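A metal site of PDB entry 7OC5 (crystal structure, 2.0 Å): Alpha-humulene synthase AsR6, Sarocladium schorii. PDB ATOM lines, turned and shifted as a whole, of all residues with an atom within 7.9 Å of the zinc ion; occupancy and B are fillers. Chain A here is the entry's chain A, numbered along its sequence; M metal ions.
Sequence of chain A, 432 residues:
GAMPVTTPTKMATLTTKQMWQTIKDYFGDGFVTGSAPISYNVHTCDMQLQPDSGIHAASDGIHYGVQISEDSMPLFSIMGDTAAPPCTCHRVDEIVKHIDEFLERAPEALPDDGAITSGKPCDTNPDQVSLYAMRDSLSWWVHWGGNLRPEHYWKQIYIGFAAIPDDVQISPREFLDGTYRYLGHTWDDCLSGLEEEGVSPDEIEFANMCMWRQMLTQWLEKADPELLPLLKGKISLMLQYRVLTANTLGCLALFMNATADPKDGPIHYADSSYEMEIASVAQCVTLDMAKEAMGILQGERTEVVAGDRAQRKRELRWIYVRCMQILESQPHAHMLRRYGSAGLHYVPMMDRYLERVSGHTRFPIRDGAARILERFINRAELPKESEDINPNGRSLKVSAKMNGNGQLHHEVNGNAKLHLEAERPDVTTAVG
ND1 of His 43 sits at hydrogen-bond distance from OD2 of Asp 46. The backbone NH of Cys 89 lies within hydrogen-bond range of the side-chain hydroxyl of Ser 236 (3.4 Å).
Of the 15 residues printed, 4 come within 4 Å of the zinc ion. The nearest printed residue that does not touch the zinc ion is Ser 236 (4.3 Å).
NE2 of His 43 binds the zinc ion, at 2.1 Å. The side-chain sulfur (SG) of Cys 89 is bound to the zinc ion. The zinc ion is bound by SG of Cys 87 (2.3 Å). SG of Cys 45 binds the zinc ion.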
ATOM      1  N   PHE A  31      -2.819 -13.461 -19.778  1.00  0.00           N
ATOM      2  CA  PHE A  31      -3.425 -12.325 -19.097  1.00  0.00           C
ATOM      3  C   PHE A  31      -2.885 -10.985 -19.582  1.00  0.00           C
ATOM      4  O   PHE A  31      -3.434  -9.947 -19.188  1.00  0.00           O
ATOM      5  CB  PHE A  31      -3.234 -12.456 -17.578  1.00  0.00           C
ATOM      6  CG  PHE A  31      -1.801 -12.463 -17.132  1.00  0.00           C
ATOM      7  CD1 PHE A  31      -1.087 -13.648 -17.036  1.00  0.00           C
ATOM      8  CD2 PHE A  31      -1.162 -11.272 -16.810  1.00  0.00           C
ATOM      9  CE1 PHE A  31       0.234 -13.658 -16.628  1.00  0.00           C
ATOM     10  CE2 PHE A  31       0.160 -11.276 -16.394  1.00  0.00           C
ATOM     11  CZ  PHE A  31       0.863 -12.471 -16.314  1.00  0.00           C
ATOM     12  N   VAL A  32      -1.852 -10.976 -20.420  1.00  0.00           N
ATOM     13  CA  VAL A  32      -1.334  -9.748 -21.023  1.00  0.00           C
ATOM     14  C   VAL A  32      -1.593  -9.802 -22.523  1.00  0.00           C
ATOM     15  O   VAL A  32      -1.369 -10.836 -23.170  1.00  0.00           O
ATOM     16  CB  VAL A  32       0.164  -9.570 -20.727  1.00  0.00           C
ATOM     17  CG1 VAL A  32       0.791  -8.608 -21.738  1.00  0.00           C
ATOM     18  CG2 VAL A  32       0.364  -9.058 -19.305  1.00  0.00           C
ATOM     19  N   VAL A  42      -3.059 -17.619 -15.825  1.00  0.00           N
ATOM     20  CA  VAL A  42      -2.969 -17.208 -14.425  1.00  0.00           C
ATOM     21  C   VAL A  42      -1.785 -16.290 -14.229  1.00  0.00           C
ATOM     22  O   VAL A  42      -0.717 -16.486 -14.829  1.00  0.00           O
ATOM     23  CB  VAL A  42      -2.870 -18.446 -13.504  1.00  0.00           C
ATOM     24  CG1 VAL A  42      -1.543 -19.149 -13.710  1.00  0.00           C
ATOM     25  CG2 VAL A  42      -3.050 -18.033 -12.062  1.00  0.00           C
ATOM     26  N   HIS A  43      -1.958 -15.274 -13.383  1.00  0.00           N
ATOM     27  CA  HIS A  43      -0.908 -14.316 -13.036  1.00  0.00           C
ATOM     28  C   HIS A  43      -0.444 -14.634 -11.619  1.00  0.00           C
ATOM     29  O   HIS A  43      -1.110 -14.286 -10.647  1.00  0.00           O
ATOM     30  CB  HIS A  43      -1.428 -12.887 -13.139  1.00  0.00           C
ATOM     31  CG  HIS A  43      -0.373 -11.837 -12.996  1.00  0.00           C
ATOM     32  ND1 HIS A  43      -0.668 -10.527 -12.703  1.00  0.00           N
ATOM     33  CD2 HIS A  43       0.975 -11.902 -13.104  1.00  0.00           C
ATOM     34  CE1 HIS A  43       0.444  -9.821 -12.639  1.00  0.00           C
ATOM     35  NE2 HIS A  43       1.459 -10.640 -12.876  1.00  0.00           N
ATOM     36  N   THR A  44       0.711 -15.292 -11.506  1.00  0.00           N
ATOM     37  CA  THR A  44       1.192 -15.733 -10.201  1.00  0.00           C
ATOM     38  C   THR A  44       1.526 -14.573  -9.273  1.00  0.00           C
ATOM     39  O   THR A  44       1.499 -14.738  -8.051  1.00  0.00           O
ATOM     40  CB  THR A  44       2.410 -16.646 -10.357  1.00  0.00           C
ATOM     41  OG1 THR A  44       3.425 -15.979 -11.109  1.00  0.00           O
ATOM     42  CG2 THR A  44       2.027 -17.934 -11.066  1.00  0.00           C
ATOM     43  N   CYS A  45       1.839 -13.393  -9.828  1.00  0.00           N
ATOM     44  CA  CYS A  45       2.161 -12.245  -8.975  1.00  0.00           C
ATOM     45  C   CYS A  45       0.978 -11.830  -8.114  1.00  0.00           C
ATOM     46  O   CYS A  45       1.178 -11.146  -7.104  1.00  0.00           O
ATOM     47  CB  CYS A  45       2.630 -11.074  -9.835  1.00  0.00           C
ATOM     48  SG  CYS A  45       4.111 -11.396 -10.827  1.00  0.00           S
ATOM     49  N   ASP A  46      -0.240 -12.226  -8.468  1.00  0.00           N
ATOM     50  CA  ASP A  46      -1.438 -11.831  -7.749  1.00  0.00           C
ATOM     51  C   ASP A  46      -1.880 -12.858  -6.721  1.00  0.00           C
ATOM     52  O   ASP A  46      -2.951 -12.697  -6.122  1.00  0.00           O
ATOM     53  CB  ASP A  46      -2.572 -11.554  -8.728  1.00  0.00           C
ATOM     54  CG  ASP A  46      -2.276 -10.397  -9.650  1.00  0.00           C
ATOM     55  OD1 ASP A  46      -1.428  -9.554  -9.283  1.00  0.00           O
ATOM     56  OD2 ASP A  46      -2.880 -10.335 -10.744  1.00  0.00           O
ATOM     57  N   PRO A  85       7.863 -11.353  -5.494  1.00  0.00           N
ATOM     58  CA  PRO A  85       8.716 -10.963  -6.615  1.00  0.00           C
ATOM     59  C   PRO A  85       8.236  -9.663  -7.236  1.00  0.00           C
ATOM     60  O   PRO A  85       7.056  -9.311  -7.124  1.00  0.00           O
ATOM     61  CB  PRO A  85       8.571 -12.138  -7.597  1.00  0.00           C
ATOM     62  CG  PRO A  85       7.210 -12.661  -7.343  1.00  0.00           C
ATOM     63  CD  PRO A  85       6.978 -12.485  -5.848  1.00  0.00           C
ATOM     64  N   PRO A  86       9.130  -8.918  -7.886  1.00  0.00           N
ATOM     65  CA  PRO A  86       8.668  -7.813  -8.728  1.00  0.00           C
ATOM     66  C   PRO A  86       8.006  -8.352  -9.976  1.00  0.00           C
ATOM     67  O   PRO A  86       8.360  -9.419 -10.492  1.00  0.00           O
ATOM     68  CB  PRO A  86       9.952  -7.037  -9.045  1.00  0.00           C
ATOM     69  CG  PRO A  86      11.033  -8.056  -8.941  1.00  0.00           C
ATOM     70  CD  PRO A  86      10.596  -9.034  -7.875  1.00  0.00           C
ATOM     71  N   CYS A  87       7.013  -7.612 -10.455  1.00  0.00           N
ATOM     72  CA  CYS A  87       6.234  -8.027 -11.621  1.00  0.00           C
ATOM     73  C   CYS A  87       6.811  -7.346 -12.863  1.00  0.00           C
ATOM     74  O   CYS A  87       6.742  -6.126 -13.008  1.00  0.00           O
ATOM     75  CB  CYS A  87       4.763  -7.675 -11.438  1.00  0.00           C
ATOM     76  SG  CYS A  87       3.806  -8.105 -12.904  1.00  0.00           S
ATOM     77  N   THR A  88       7.364  -8.155 -13.766  1.00  0.00           N
ATOM     78  CA  THR A  88       7.777  -7.717 -15.088  1.00  0.00           C
ATOM     79  C   THR A  88       6.955  -8.373 -16.189  1.00  0.00           C
ATOM     80  O   THR A  88       7.359  -8.372 -17.357  1.00  0.00           O
ATOM     81  CB  THR A  88       9.265  -7.992 -15.298  1.00  0.00           C
ATOM     82  OG1 THR A  88       9.527  -9.394 -15.133  1.00  0.00           O
ATOM     83  CG2 THR A  88      10.107  -7.208 -14.294  1.00  0.00           C
ATOM     84  N   CYS A  89       5.784  -8.923 -15.824  1.00  0.00           N
ATOM     85  CA  CYS A  89       5.020  -9.733 -16.768  1.00  0.00           C
ATOM     86  C   CYS A  89       4.487  -8.914 -17.944  1.00  0.00           C
ATOM     87  O   CYS A  89       4.298  -9.460 -19.033  1.00  0.00           O
ATOM     88  CB  CYS A  89       3.853 -10.408 -16.046  1.00  0.00           C
ATOM     89  SG  CYS A  89       4.329 -11.543 -14.720  1.00  0.00           S
ATOM     90  N   HIS A  90       4.240  -7.620 -17.741  1.00  0.00           N
ATOM     91  CA  HIS A  90       3.686  -6.811 -18.825  1.00  0.00           C
ATOM     92  C   HIS A  90       4.671  -6.617 -19.972  1.00  0.00           C
ATOM     93  O   HIS A  90       4.268  -6.140 -21.030  1.00  0.00           O
ATOM     94  CB  HIS A  90       3.240  -5.449 -18.291  1.00  0.00           C
ATOM     95  CG  HIS A  90       1.861  -5.457 -17.714  1.00  0.00           C
ATOM     96  ND1 HIS A  90       1.591  -5.872 -16.429  1.00  0.00           N
ATOM     97  CD2 HIS A  90       0.671  -5.108 -18.245  1.00  0.00           C
ATOM     98  CE1 HIS A  90       0.298  -5.775 -16.190  1.00  0.00           C
ATOM     99  NE2 HIS A  90      -0.288  -5.308 -17.287  1.00  0.00           N
ATOM    100  N   SER A 236       9.775 -12.857 -13.107  1.00  0.00           N
ATOM    101  CA  SER A 236       8.422 -13.316 -13.410  1.00  0.00           C
ATOM    102  C   SER A 236       8.324 -13.795 -14.860  1.00  0.00           C
ATOM    103  O   SER A 236       7.634 -14.787 -15.141  1.00  0.00           O
ATOM    104  CB  SER A 236       7.406 -12.200 -13.139  1.00  0.00           C
ATOM    105  OG  SER A 236       7.598 -11.087 -13.976  1.00  0.00           O
ATOM    106  N   LEU A 237       9.025 -13.133 -15.789  1.00  0.00           N
ATOM    107  CA  LEU A 237       9.032 -13.587 -17.168  1.00  0.00           C
ATOM    108  C   LEU A 237       9.896 -14.837 -17.352  1.00  0.00           C
ATOM    109  O   LEU A 237       9.549 -15.730 -18.131  1.00  0.00           O
ATOM    110  CB  LEU A 237       9.544 -12.473 -18.090  1.00  0.00           C
ATOM    111  CG  LEU A 237       8.592 -11.331 -18.428  1.00  0.00           C
ATOM    112  CD1 LEU A 237       9.309 -10.295 -19.279  1.00  0.00           C
ATOM    113  CD2 LEU A 237       7.349 -11.830 -19.143  1.00  0.00           C
HETATM  114 ZN    ZN M   1       3.519 -10.415 -12.857  1.00  0.00          ZN
